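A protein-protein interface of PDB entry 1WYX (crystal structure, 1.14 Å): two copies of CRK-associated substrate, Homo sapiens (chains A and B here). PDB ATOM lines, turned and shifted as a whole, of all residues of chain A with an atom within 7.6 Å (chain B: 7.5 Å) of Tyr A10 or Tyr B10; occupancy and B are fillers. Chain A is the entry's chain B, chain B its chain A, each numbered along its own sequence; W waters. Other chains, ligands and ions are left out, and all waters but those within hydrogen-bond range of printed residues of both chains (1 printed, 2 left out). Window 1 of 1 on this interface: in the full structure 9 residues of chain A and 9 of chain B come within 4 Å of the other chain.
O of Arg B57 is in hydrogen-bond range of N of Leu B9 (2.8 Å). O of Tyr B10 is in hydrogen-bond range of N of Lys B24 (3.5 Å). OD2 of Asp B11 is in hydrogen-bond range of N of Lys B24, at 2.8 Å. The backbone carbonyl oxygen (O) of Asp B11 sits at hydrogen-bond distance from the guanidinium group (NH1) of Arg B57. The backbone carbonyl oxygen (O) of Arg A57 is in hydrogen-bond range of the backbone NH (N) of Leu A9 (2.8 Å). The backbone carbonyl oxygen (O) of Asp A11 lies within hydrogen-bond range of the guanidinium group (NH1) of Arg A57.
Of the 16 printed residues of chain B, 8 touch a printed residue of chain A. Printed residues of chain B that touch a printed residue of chain A: Tyr B10, Asp B11, Asn B12, Val B13, Phe B22, Arg B23, Lys B24 and Arg B57. Hydrophobic or aromatic side chains of chain B within 4 Å of the printed part of chain A: Tyr B10 and Val B13. Of the 18 printed residues of chain A, 6 touch a printed residue of chain B. Hydrophobic or aromatic side chains of chain A within 4 Å of the printed part of chain B: Tyr A10 and Val A13. Along chain A the printed residues that touch a printed residue of chain B span positions 10 to 57. Among the printed residues, 15 pairs touch across the chains. Among the printed residues, Asp or Glu carboxylates within 4 Å of a Lys or Arg side-chain nitrogen of the other chain: Asp A11 with Arg B57 (3.3 Å) and Arg A57 with Asp B11 (3.0 Å).
Tyr B10 touches its own counterpart, Tyr A10. Asn A12 touches Val B13, and with the chains exchanged Val A13 touches Asn B12. Val A13 touches Phe B22, and with the chains exchanged Phe A22 touches Val B13. Arg A57 touches Lys B24, but with the chains exchanged Lys A24 does not touch Arg B57 (6.5 Å). Positions printed for both chains: 7, 8, 9, 10, 11, 12, 13, 22, 23, 24, 25, 26, 28, 56, 57 and 58.
Water W1 lies within hydrogen-bond range of the side-chain carboxylate of Asp A11 and the guanidinium group of Arg B57.
The backbone NH (N) of Val A13 sits at hydrogen-bond distance from the side-chain carboxylate (OD1) of Asp B11, at 2.9 Å. NH2 of Arg A57 lies within salt-bridge range of OD2 of Asp B11. OD1 of Asp A11 lies within hydrogen-bond range of N of Val B13 (3.0 Å). The guanidinium group of Arg B23 lies within hydrogen-bond range of the backbone carbonyl oxygen of Val A13 (3.1 Å). The guanidinium group of Arg B57 lies within salt-bridge range of the side-chain carboxylate of Asp A11 (3.3 Å).
Among the printed residues, merely in contact across the chains: Val A13 with Asn B12 (3.2 Å), Phe A22 with Val B13 (3.4 Å), Val A13 with Phe B22 (3.5 Å), Asp A11 with Asp B11 (3.5 Å), Asn A12 with Asp B11 (3.5 Å), Asp A11 with Asn B12 (3.7 Å), Asn A12 with Val B13 (3.7 Å), Val A13 with Val B13 (3.8 Å), Arg A57 with Lys B24 (3.9 Å) and Tyr A10 with Tyr B10 (3.996 Å).
Printed residues of chain B within 4 Å of Tyr A10: Tyr B10 (3.996 Å). Of the printed residues of chain B, Asn A12 touches Asp B11 and Val B13. Of the printed residues of chain A, Tyr B10 touches Tyr A10 (3.996 Å). Printed residues of chain A within 4 Å of Asn B12: Asp A11 and Val A13. Printed residues of chain A within 4 Å of Val B13: Asp A11, Asn A12, Val A13 and Phe A22. Of the printed residues of chain A, Arg B57 touches Asp A11. The nearest printed residue of chain A that does not touch Tyr B10 is Arg A57 (5.1 Å). The nearest printed residue of chain A that does not touch Asp B11 is Tyr A10 (6.0 Å).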
ATOM      1  N   LYS A   7     -16.799 -25.078  14.627  1.00  0.00           N
ATOM      2  CA  LYS A   7     -17.522 -24.294  15.618  1.00  0.00           C
ATOM      3  C   LYS A   7     -17.734 -22.890  15.078  1.00  0.00           C
ATOM      4  O   LYS A   7     -16.824 -22.265  14.537  1.00  0.00           O
ATOM      5  CB  LYS A   7     -16.738 -24.241  16.924  1.00  0.00           C
ATOM      6  CG  LYS A   7     -17.408 -23.483  18.065  1.00  0.00           C
ATOM      7  CD  LYS A   7     -16.536 -23.629  19.307  1.00  0.00           C
ATOM      8  CE  LYS A   7     -17.097 -22.993  20.549  1.00  0.00           C
ATOM      9  NZ  LYS A   7     -16.224 -23.334  21.702  1.00  0.00           N
ATOM     10  N   ALA A   8     -18.951 -22.389  15.246  1.00  0.00           N
ATOM     11  CA  ALA A   8     -19.305 -21.041  14.845  1.00  0.00           C
ATOM     12  C   ALA A   8     -18.613 -20.007  15.736  1.00  0.00           C
ATOM     13  O   ALA A   8     -18.712 -20.052  16.956  1.00  0.00           O
ATOM     14  CB  ALA A   8     -20.805 -20.859  14.925  1.00  0.00           C
ATOM     15  N   LEU A   9     -17.930 -19.074  15.094  1.00  0.00           N
ATOM     16  CA  LEU A   9     -17.292 -17.918  15.747  1.00  0.00           C
ATOM     17  C   LEU A   9     -18.241 -16.741  15.912  1.00  0.00           C
ATOM     18  O   LEU A   9     -17.941 -15.809  16.650  1.00  0.00           O
ATOM     19  CB  LEU A   9     -16.110 -17.465  14.896  1.00  0.00           C
ATOM     20  CG  LEU A   9     -15.024 -18.508  14.665  1.00  0.00           C
ATOM     21  CD1 LEU A   9     -14.043 -18.046  13.616  1.00  0.00           C
ATOM     22  CD2 LEU A   9     -14.340 -18.786  15.951  1.00  0.00           C
ATOM     23  N   TYR A  10     -19.345 -16.772  15.173  1.00  0.00           N
ATOM     24  CA  TYR A  10     -20.306 -15.679  15.101  1.00  0.00           C
ATOM     25  C   TYR A  10     -21.694 -16.266  14.910  1.00  0.00           C
ATOM     26  O   TYR A  10     -21.842 -17.422  14.492  1.00  0.00           O
ATOM     27  CB  TYR A  10     -19.991 -14.789  13.894  1.00  0.00           C
ATOM     28  CG  TYR A  10     -18.576 -14.261  13.839  1.00  0.00           C
ATOM     29  CD1 TYR A  10     -17.597 -14.876  13.066  1.00  0.00           C
ATOM     30  CD2 TYR A  10     -18.222 -13.124  14.552  1.00  0.00           C
ATOM     31  CE1 TYR A  10     -16.295 -14.377  13.022  1.00  0.00           C
ATOM     32  CE2 TYR A  10     -16.936 -12.627  14.518  1.00  0.00           C
ATOM     33  CZ  TYR A  10     -15.977 -13.250  13.752  1.00  0.00           C
ATOM     34  OH  TYR A  10     -14.696 -12.741  13.713  1.00  0.00           O
ATOM     35  N   ASP A  11     -22.714 -15.463  15.188  1.00  0.00           N
ATOM     36  CA  ASP A  11     -24.071 -15.755  14.745  1.00  0.00           C
ATOM     37  C   ASP A  11     -24.149 -15.657  13.232  1.00  0.00           C
ATOM     38  O   ASP A  11     -23.364 -14.970  12.598  1.00  0.00           O
ATOM     39  CB  ASP A  11     -25.075 -14.733  15.304  1.00  0.00           C
ATOM     40  CG  ASP A  11     -25.352 -14.897  16.770  1.00  0.00           C
ATOM     41  OD1 ASP A  11     -26.221 -14.133  17.288  1.00  0.00           O
ATOM     42  OD2 ASP A  11     -24.777 -15.728  17.496  1.00  0.00           O
ATOM     43  N   ASN A  12     -25.146 -16.325  12.663  1.00  0.00           N
ATOM     44  CA  ASN A  12     -25.441 -16.251  11.255  1.00  0.00           C
ATOM     45  C   ASN A  12     -26.947 -16.321  11.054  1.00  0.00           C
ATOM     46  O   ASN A  12     -27.585 -17.276  11.478  1.00  0.00           O
ATOM     47  CB  ASN A  12     -24.744 -17.377  10.509  1.00  0.00           C
ATOM     48  CG  ASN A  12     -24.761 -17.171   9.017  1.00  0.00           C
ATOM     49  OD1 ASN A  12     -24.074 -16.292   8.492  1.00  0.00           O
ATOM     50  ND2 ASN A  12     -25.525 -17.985   8.314  1.00  0.00           N
ATOM     51  N   VAL A  13     -27.507 -15.287  10.436  1.00  0.00           N
ATOM     52  CA  VAL A  13     -28.933 -15.207  10.156  1.00  0.00           C
ATOM     53  C   VAL A  13     -29.130 -15.488   8.669  1.00  0.00           C
ATOM     54  O   VAL A  13     -28.748 -14.694   7.821  1.00  0.00           O
ATOM     55  CB  VAL A  13     -29.513 -13.824  10.544  1.00  0.00           C
ATOM     56  CG1 VAL A  13     -30.942 -13.656  10.025  1.00  0.00           C
ATOM     57  CG2 VAL A  13     -29.471 -13.619  12.052  1.00  0.00           C
ATOM     58  N   PHE A  22     -27.403 -20.008  12.598  1.00  0.00           N
ATOM     59  CA  PHE A  22     -26.753 -20.583  13.761  1.00  0.00           C
ATOM     60  C   PHE A  22     -26.286 -19.492  14.686  1.00  0.00           C
ATOM     61  O   PHE A  22     -26.252 -18.306  14.337  1.00  0.00           O
ATOM     62  CB  PHE A  22     -25.602 -21.526  13.366  1.00  0.00           C
ATOM     63  CG  PHE A  22     -24.579 -20.919  12.451  1.00  0.00           C
ATOM     64  CD1 PHE A  22     -23.531 -20.136  12.954  1.00  0.00           C
ATOM     65  CD2 PHE A  22     -24.650 -21.139  11.084  1.00  0.00           C
ATOM     66  CE1 PHE A  22     -22.565 -19.623  12.117  1.00  0.00           C
ATOM     67  CE2 PHE A  22     -23.701 -20.616  10.241  1.00  0.00           C
ATOM     68  CZ  PHE A  22     -22.647 -19.850  10.760  1.00  0.00           C
ATOM     69  N   ARG A  23     -25.917 -19.911  15.885  1.00  0.00           N
ATOM     70  CA  ARG A  23     -25.403 -19.009  16.890  1.00  0.00           C
ATOM     71  C   ARG A  23     -23.943 -19.274  17.165  1.00  0.00           C
ATOM     72  O   ARG A  23     -23.480 -20.413  17.048  1.00  0.00           O
ATOM     73  CB  ARG A  23     -26.169 -19.221  18.180  1.00  0.00           C
ATOM     74  CG  ARG A  23     -27.627 -18.850  18.096  1.00  0.00           C
ATOM     75  CD  ARG A  23     -28.410 -19.186  19.342  1.00  0.00           C
ATOM     76  NE  ARG A  23     -28.305 -20.601  19.681  1.00  0.00           N
ATOM     77  CZ  ARG A  23     -28.928 -21.191  20.699  1.00  0.00           C
ATOM     78  NH1 ARG A  23     -29.739 -20.501  21.493  1.00  0.00           N
ATOM     79  NH2 ARG A  23     -28.746 -22.489  20.917  1.00  0.00           N
ATOM     80  N   LYS A  24     -23.243 -18.229  17.611  1.00  0.00           N
ATOM     81  CA  LYS A  24     -21.883 -18.372  18.075  1.00  0.00           C
ATOM     82  C   LYS A  24     -21.798 -19.547  19.058  1.00  0.00           C
ATOM     83  O   LYS A  24     -22.596 -19.668  19.986  1.00  0.00           O
ATOM     84  CB  LYS A  24     -21.414 -17.081  18.744  1.00  0.00           C
ATOM     85  CG  LYS A  24     -19.978 -17.139  19.202  1.00  0.00           C
ATOM     86  CD  LYS A  24     -19.487 -15.804  19.746  1.00  0.00           C
ATOM     87  CE  LYS A  24     -18.039 -15.904  20.207  1.00  0.00           C
ATOM     88  NZ  LYS A  24     -17.520 -14.618  20.764  1.00  0.00           N
ATOM     89  N   GLY A  25     -20.818 -20.417  18.849  1.00  0.00           N
ATOM     90  CA  GLY A  25     -20.618 -21.573  19.696  1.00  0.00           C
ATOM     91  C   GLY A  25     -21.231 -22.863  19.175  1.00  0.00           C
ATOM     92  O   GLY A  25     -20.884 -23.939  19.662  1.00  0.00           O
ATOM     93  N   ASP A  26     -22.156 -22.781  18.220  1.00  0.00           N
ATOM     94  CA  ASP A  26     -22.733 -23.996  17.649  1.00  0.00           C
ATOM     95  C   ASP A  26     -21.664 -24.829  16.970  1.00  0.00           C
ATOM     96  O   ASP A  26     -20.769 -24.297  16.312  1.00  0.00           O
ATOM     97  CB  ASP A  26     -23.836 -23.681  16.645  1.00  0.00           C
ATOM     98  CG  ASP A  26     -25.119 -23.236  17.307  1.00  0.00           C
ATOM     99  OD1 ASP A  26     -26.002 -22.700  16.604  1.00  0.00           O
ATOM    100  OD2 ASP A  26     -25.310 -23.360  18.537  1.00  0.00           O
ATOM    101  N   MET A  28     -21.062 -27.770  14.168  1.00  0.00           N
ATOM    102  CA  MET A  28     -21.698 -28.349  13.000  1.00  0.00           C
ATOM    103  C   MET A  28     -20.727 -29.242  12.251  1.00  0.00           C
ATOM    104  O   MET A  28     -19.509 -29.136  12.385  1.00  0.00           O
ATOM    105  CB  MET A  28     -22.235 -27.247  12.094  1.00  0.00           C
ATOM    106  CG  MET A  28     -21.179 -26.347  11.489  1.00  0.00           C
ATOM    107  SD  MET A  28     -21.850 -24.801  10.804  1.00  0.00           S
ATOM    108  CE  MET A  28     -22.181 -23.878  12.324  1.00  0.00           C
ATOM    109  N   PRO A  54     -21.142 -19.446   5.532  1.00  0.00           N
ATOM    110  CA  PRO A  54     -19.870 -18.812   5.192  1.00  0.00           C
ATOM    111  C   PRO A  54     -18.736 -19.439   6.006  1.00  0.00           C
ATOM    112  O   PRO A  54     -18.740 -19.352   7.233  1.00  0.00           O
ATOM    113  CB  PRO A  54     -20.089 -17.331   5.558  1.00  0.00           C
ATOM    114  CG  PRO A  54     -21.549 -17.182   5.620  1.00  0.00           C
ATOM    115  CD  PRO A  54     -22.055 -18.502   6.195  1.00  0.00           C
ATOM    116  N   ASN A  56     -15.790 -18.517   6.575  1.00  0.00           N
ATOM    117  CA  ASN A  56     -15.014 -17.591   7.396  1.00  0.00           C
ATOM    118  C   ASN A  56     -15.686 -17.237   8.725  1.00  0.00           C
ATOM    119  O   ASN A  56     -15.091 -16.539   9.538  1.00  0.00           O
ATOM    120  CB  ASN A  56     -14.577 -16.334   6.625  1.00  0.00           C
ATOM    121  CG  ASN A  56     -15.721 -15.483   6.122  1.00  0.00           C
ATOM    122  OD1 ASN A  56     -15.500 -14.583   5.288  1.00  0.00           O
ATOM    123  ND2 ASN A  56     -16.914 -15.712   6.602  1.00  0.00           N
ATOM    124  N   ARG A  57     -16.890 -17.749   8.979  1.00  0.00           N
ATOM    125  CA  ARG A  57     -17.531 -17.614  10.278  1.00  0.00           C
ATOM    126  C   ARG A  57     -17.323 -18.824  11.183  1.00  0.00           C
ATOM    127  O   ARG A  57     -17.885 -18.866  12.271  1.00  0.00           O
ATOM    128  CB  ARG A  57     -19.015 -17.343  10.088  1.00  0.00           C
ATOM    129  CG  ARG A  57     -19.225 -15.994   9.401  1.00  0.00           C
ATOM    130  CD  ARG A  57     -20.613 -15.693   8.958  1.00  0.00           C
ATOM    131  NE  ARG A  57     -20.785 -14.245   8.846  1.00  0.00           N
ATOM    132  CZ  ARG A  57     -21.710 -13.545   9.491  1.00  0.00           C
ATOM    133  NH1 ARG A  57     -22.572 -14.160  10.291  1.00  0.00           N
ATOM    134  NH2 ARG A  57     -21.778 -12.221   9.334  1.00  0.00           N
ATOM    135  N   LEU A  58     -16.491 -19.767  10.744  1.00  0.00           N
ATOM    136  CA  LEU A  58     -16.237 -21.013  11.467  1.00  0.00           C
ATOM    137  C   LEU A  58     -14.770 -21.142  11.834  1.00  0.00           C
ATOM    138  O   LEU A  58     -13.892 -20.529  11.208  1.00  0.00           O
ATOM    139  CB  LEU A  58     -16.592 -22.224  10.603  1.00  0.00           C
ATOM    140  CG  LEU A  58     -17.999 -22.255  10.027  1.00  0.00           C
ATOM    141  CD1 LEU A  58     -18.173 -23.481   9.137  1.00  0.00           C
ATOM    142  CD2 LEU A  58     -19.064 -22.202  11.114  1.00  0.00           C
ATOM    143  N   LYS A  59     -14.497 -21.969  12.834  1.00  0.00           N
ATOM    144  CA  LYS A  59     -13.165 -22.535  13.001  1.00  0.00           C
ATOM    145  C   LYS A  59     -13.260 -24.052  13.025  1.00  0.00           C
ATOM    146  O   LYS A  59     -14.201 -24.629  13.577  1.00  0.00           O
ATOM    147  CB  LYS A  59     -12.458 -22.012  14.246  1.00  0.00           C
ATOM    148  CG  LYS A  59     -13.099 -22.412  15.534  1.00  0.00           C
ATOM    149  CD  LYS A  59     -12.257 -21.993  16.742  1.00  0.00           C
ATOM    150  CE  LYS A  59     -12.907 -22.495  18.030  1.00  0.00           C
ATOM    151  NZ  LYS A  59     -12.227 -21.993  19.261  1.00  0.00           N
ATOM    152  N   LYS B   7     -25.127   0.890  11.953  1.00  0.00           N
ATOM    153  CA  LYS B   7     -24.892  -0.272  11.122  1.00  0.00           C
ATOM    154  C   LYS B   7     -24.521  -1.486  11.973  1.00  0.00           C
ATOM    155  O   LYS B   7     -23.714  -1.386  12.899  1.00  0.00           O
ATOM    156  CB  LYS B   7     -23.765   0.047  10.152  1.00  0.00           C
ATOM    157  CG  LYS B   7     -23.396  -1.075   9.208  1.00  0.00           C
ATOM    158  CD  LYS B   7     -22.426  -0.609   8.136  1.00  0.00           C
ATOM    159  CE  LYS B   7     -21.066  -0.271   8.696  1.00  0.00           C
ATOM    160  NZ  LYS B   7     -20.125   0.169   7.617  1.00  0.00           N
ATOM    161  N   ALA B   8     -25.068  -2.645  11.618  1.00  0.00           N
ATOM    162  CA  ALA B   8     -24.730  -3.885  12.296  1.00  0.00           C
ATOM    163  C   ALA B   8     -23.302  -4.318  11.952  1.00  0.00           C
ATOM    164  O   ALA B   8     -22.931  -4.436  10.784  1.00  0.00           O
ATOM    165  CB  ALA B   8     -25.707  -4.966  11.919  1.00  0.00           C
ATOM    166  N   LEU B   9     -22.512  -4.584  12.985  1.00  0.00           N
ATOM    167  CA  LEU B   9     -21.156  -5.099  12.822  1.00  0.00           C
ATOM    168  C   LEU B   9     -21.125  -6.619  12.743  1.00  0.00           C
ATOM    169  O   LEU B   9     -20.095  -7.198  12.388  1.00  0.00           O
ATOM    170  CB  LEU B   9     -20.289  -4.625  13.990  1.00  0.00           C
ATOM    171  CG  LEU B   9     -20.098  -3.109  14.043  1.00  0.00           C
ATOM    172  CD1 LEU B   9     -19.390  -2.710  15.328  1.00  0.00           C
ATOM    173  CD2 LEU B   9     -19.323  -2.675  12.823  1.00  0.00           C
ATOM    174  N   TYR B  10     -22.240  -7.243  13.106  1.00  0.00           N
ATOM    175  CA  TYR B  10     -22.386  -8.691  13.207  1.00  0.00           C
ATOM    176  C   TYR B  10     -23.788  -9.072  12.804  1.00  0.00           C
ATOM    177  O   TYR B  10     -24.713  -8.253  12.884  1.00  0.00           O
ATOM    178  CB  TYR B  10     -22.216  -9.146  14.662  1.00  0.00           C
ATOM    179  CG  TYR B  10     -20.924  -8.728  15.299  1.00  0.00           C
ATOM    180  CD1 TYR B  10     -20.828  -7.548  16.030  1.00  0.00           C
ATOM    181  CD2 TYR B  10     -19.782  -9.491  15.134  1.00  0.00           C
ATOM    182  CE1 TYR B  10     -19.629  -7.157  16.596  1.00  0.00           C
ATOM    183  CE2 TYR B  10     -18.586  -9.118  15.701  1.00  0.00           C
ATOM    184  CZ  TYR B  10     -18.512  -7.948  16.428  1.00  0.00           C
ATOM    185  OH  TYR B  10     -17.305  -7.586  16.977  1.00  0.00           O
ATOM    186  N   ASP B  11     -23.983 -10.335  12.450  1.00  0.00           N
ATOM    187  CA  ASP B  11     -25.329 -10.883  12.414  1.00  0.00           C
ATOM    188  C   ASP B  11     -25.773 -11.080  13.850  1.00  0.00           C
ATOM    189  O   ASP B  11     -24.949 -11.223  14.758  1.00  0.00           O
ATOM    190  CB  ASP B  11     -25.389 -12.261  11.759  1.00  0.00           C
ATOM    191  CG  ASP B  11     -25.270 -12.227  10.253  1.00  0.00           C
ATOM    192  OD1 ASP B  11     -25.769 -13.183   9.607  1.00  0.00           O
ATOM    193  OD2 ASP B  11     -24.675 -11.332   9.620  1.00  0.00           O
ATOM    194  N   ASN B  12     -27.084 -11.138  14.052  1.00  0.00           N
ATOM    195  CA  ASN B  12     -27.638 -11.344  15.379  1.00  0.00           C
ATOM    196  C   ASN B  12     -28.889 -12.195  15.309  1.00  0.00           C
ATOM    197  O   ASN B  12     -29.874 -11.805  14.708  1.00  0.00           O
ATOM    198  CB  ASN B  12     -27.981  -9.988  16.015  1.00  0.00           C
ATOM    199  CG  ASN B  12     -28.412 -10.106  17.477  1.00  0.00           C
ATOM    200  OD1 ASN B  12     -27.571 -10.289  18.377  1.00  0.00           O
ATOM    201  ND2 ASN B  12     -29.720  -9.989  17.728  1.00  0.00           N
ATOM    202  N   VAL B  13     -28.817 -13.382  15.902  1.00  0.00           N
ATOM    203  CA  VAL B  13     -29.959 -14.266  16.025  1.00  0.00           C
ATOM    204  C   VAL B  13     -30.763 -13.874  17.260  1.00  0.00           C
ATOM    205  O   VAL B  13     -30.290 -13.958  18.382  1.00  0.00           O
ATOM    206  CB  VAL B  13     -29.506 -15.740  16.114  1.00  0.00           C
ATOM    207  CG1 VAL B  13     -30.663 -16.648  16.545  1.00  0.00           C
ATOM    208  CG2 VAL B  13     -28.903 -16.171  14.768  1.00  0.00           C
ATOM    209  N   PHE B  22     -30.874  -9.618  12.721  1.00  0.00           N
ATOM    210  CA  PHE B  22     -30.325  -8.797  11.665  1.00  0.00           C
ATOM    211  C   PHE B  22     -29.024  -9.382  11.151  1.00  0.00           C
ATOM    212  O   PHE B  22     -28.477 -10.315  11.732  1.00  0.00           O
ATOM    213  CB  PHE B  22     -30.158  -7.336  12.119  1.00  0.00           C
ATOM    214  CG  PHE B  22     -29.405  -7.151  13.410  1.00  0.00           C
ATOM    215  CD1 PHE B  22     -28.018  -7.099  13.420  1.00  0.00           C
ATOM    216  CD2 PHE B  22     -30.085  -6.967  14.603  1.00  0.00           C
ATOM    217  CE1 PHE B  22     -27.332  -6.882  14.591  1.00  0.00           C
ATOM    218  CE2 PHE B  22     -29.410  -6.749  15.764  1.00  0.00           C
ATOM    219  CZ  PHE B  22     -28.025  -6.702  15.768  1.00  0.00           C
ATOM    220  N   ARG B  23     -28.558  -8.839  10.039  1.00  0.00           N
ATOM    221  CA  ARG B  23     -27.359  -9.303   9.373  1.00  0.00           C
ATOM    222  C   ARG B  23     -26.335  -8.188   9.361  1.00  0.00           C
ATOM    223  O   ARG B  23     -26.674  -6.992   9.292  1.00  0.00           O
ATOM    224  CB  ARG B  23     -27.690  -9.731   7.946  1.00  0.00           C
ATOM    225  CG  ARG B  23     -28.746 -10.819   7.900  1.00  0.00           C
ATOM    226  CD  ARG B  23     -29.019 -11.399   6.529  1.00  0.00           C
ATOM    227  NE  ARG B  23     -30.207 -12.268   6.550  1.00  0.00           N
ATOM    228  CZ  ARG B  23     -31.469 -11.862   6.408  1.00  0.00           C
ATOM    229  NH1 ARG B  23     -31.752 -10.585   6.210  1.00  0.00           N
ATOM    230  NH2 ARG B  23     -32.463 -12.739   6.468  1.00  0.00           N
ATOM    231  N   LYS B  24     -25.067  -8.574   9.428  1.00  0.00           N
ATOM    232  CA  LYS B  24     -23.969  -7.629   9.296  1.00  0.00           C
ATOM    233  C   LYS B  24     -24.203  -6.723   8.091  1.00  0.00           C
ATOM    234  O   LYS B  24     -24.550  -7.190   7.005  1.00  0.00           O
ATOM    235  CB  LYS B  24     -22.654  -8.391   9.147  1.00  0.00           C
ATOM    236  CG  LYS B  24     -21.431  -7.512   9.065  1.00  0.00           C
ATOM    237  CD  LYS B  24     -20.154  -8.336   9.004  1.00  0.00           C
ATOM    238  CE  LYS B  24     -18.920  -7.439   9.012  1.00  0.00           C
ATOM    239  NZ  LYS B  24     -17.650  -8.208   8.954  1.00  0.00           N
ATOM    240  N   GLY B  25     -24.050  -5.415   8.290  1.00  0.00           N
ATOM    241  CA  GLY B  25     -24.251  -4.450   7.233  1.00  0.00           C
ATOM    242  C   GLY B  25     -25.621  -3.816   7.229  1.00  0.00           C
ATOM    243  O   GLY B  25     -25.792  -2.760   6.628  1.00  0.00           O
ATOM    244  N   ASP B  26     -26.595  -4.425   7.895  1.00  0.00           N
ATOM    245  CA  ASP B  26     -27.918  -3.820   7.990  1.00  0.00           C
ATOM    246  C   ASP B  26     -27.836  -2.481   8.709  1.00  0.00           C
ATOM    247  O   ASP B  26     -27.110  -2.343   9.690  1.00  0.00           O
ATOM    248  CB  ASP B  26     -28.887  -4.715   8.773  1.00  0.00           C
ATOM    249  CG  ASP B  26     -29.377  -5.920   7.985  1.00  0.00           C
ATOM    250  OD1 ASP B  26     -30.005  -6.801   8.625  1.00  0.00           O
ATOM    251  OD2 ASP B  26     -29.192  -6.043   6.754  1.00  0.00           O
ATOM    252  N   MET B  28     -30.064   0.305  10.796  1.00  0.00           N
ATOM    253  CA  MET B  28     -31.289   0.470  11.547  1.00  0.00           C
ATOM    254  C   MET B  28     -31.325   1.828  12.227  1.00  0.00           C
ATOM    255  O   MET B  28     -30.291   2.486  12.443  1.00  0.00           O
ATOM    256  CB  MET B  28     -31.442  -0.664  12.563  1.00  0.00           C
ATOM    257  CG  MET B  28     -30.358  -0.705  13.628  1.00  0.00           C
ATOM    258  SD  MET B  28     -30.362  -2.260  14.544  1.00  0.00           S
ATOM    259  CE  MET B  28     -29.542  -3.331  13.345  1.00  0.00           C
ATOM    260  N   ASN B  56     -23.560  -2.964  21.546  1.00  0.00           N
ATOM    261  CA  ASN B  56     -22.230  -3.449  21.217  1.00  0.00           C
ATOM    262  C   ASN B  56     -22.170  -4.282  19.932  1.00  0.00           C
ATOM    263  O   ASN B  56     -21.095  -4.705  19.507  1.00  0.00           O
ATOM    264  CB  ASN B  56     -21.567  -4.153  22.425  1.00  0.00           C
ATOM    265  CG  ASN B  56     -22.206  -5.495  22.803  1.00  0.00           C
ATOM    266  OD1 ASN B  56     -21.939  -6.007  23.895  1.00  0.00           O
ATOM    267  ND2 ASN B  56     -22.985  -6.086  21.933  1.00  0.00           N
ATOM    268  N   ARG B  57     -23.302  -4.493  19.276  1.00  0.00           N
ATOM    269  CA  ARG B  57     -23.267  -5.079  17.945  1.00  0.00           C
ATOM    270  C   ARG B  57     -23.397  -4.072  16.831  1.00  0.00           C
ATOM    271  O   ARG B  57     -23.396  -4.451  15.671  1.00  0.00           O
ATOM    272  CB  ARG B  57     -24.303  -6.169  17.821  1.00  0.00           C
ATOM    273  CG  ARG B  57     -23.892  -7.307  18.707  1.00  0.00           C
ATOM    274  CD  ARG B  57     -24.513  -8.589  18.365  1.00  0.00           C
ATOM    275  NE  ARG B  57     -24.413  -9.526  19.476  1.00  0.00           N
ATOM    276  CZ  ARG B  57     -24.479 -10.848  19.351  1.00  0.00           C
ATOM    277  NH1 ARG B  57     -24.656 -11.410  18.159  1.00  0.00           N
ATOM    278  NH2 ARG B  57     -24.382 -11.600  20.439  1.00  0.00           N
ATOM    279  N   LEU B  58     -23.459  -2.793  17.187  1.00  0.00           N
ATOM    280  CA  LEU B  58     -23.741  -1.723  16.237  1.00  0.00           C
ATOM    281  C   LEU B  58     -22.648  -0.673  16.220  1.00  0.00           C
ATOM    282  O   LEU B  58     -21.924  -0.483  17.189  1.00  0.00           O
ATOM    283  CB  LEU B  58     -25.072  -1.045  16.590  1.00  0.00           C
ATOM    284  CG  LEU B  58     -26.301  -1.958  16.715  1.00  0.00           C
ATOM    285  CD1 LEU B  58     -27.511  -1.120  17.094  1.00  0.00           C
ATOM    286  CD2 LEU B  58     -26.568  -2.757  15.436  1.00  0.00           C
HETATM  287  O   HOH W   1     -23.282 -14.206  19.454  1.00  0.00           O
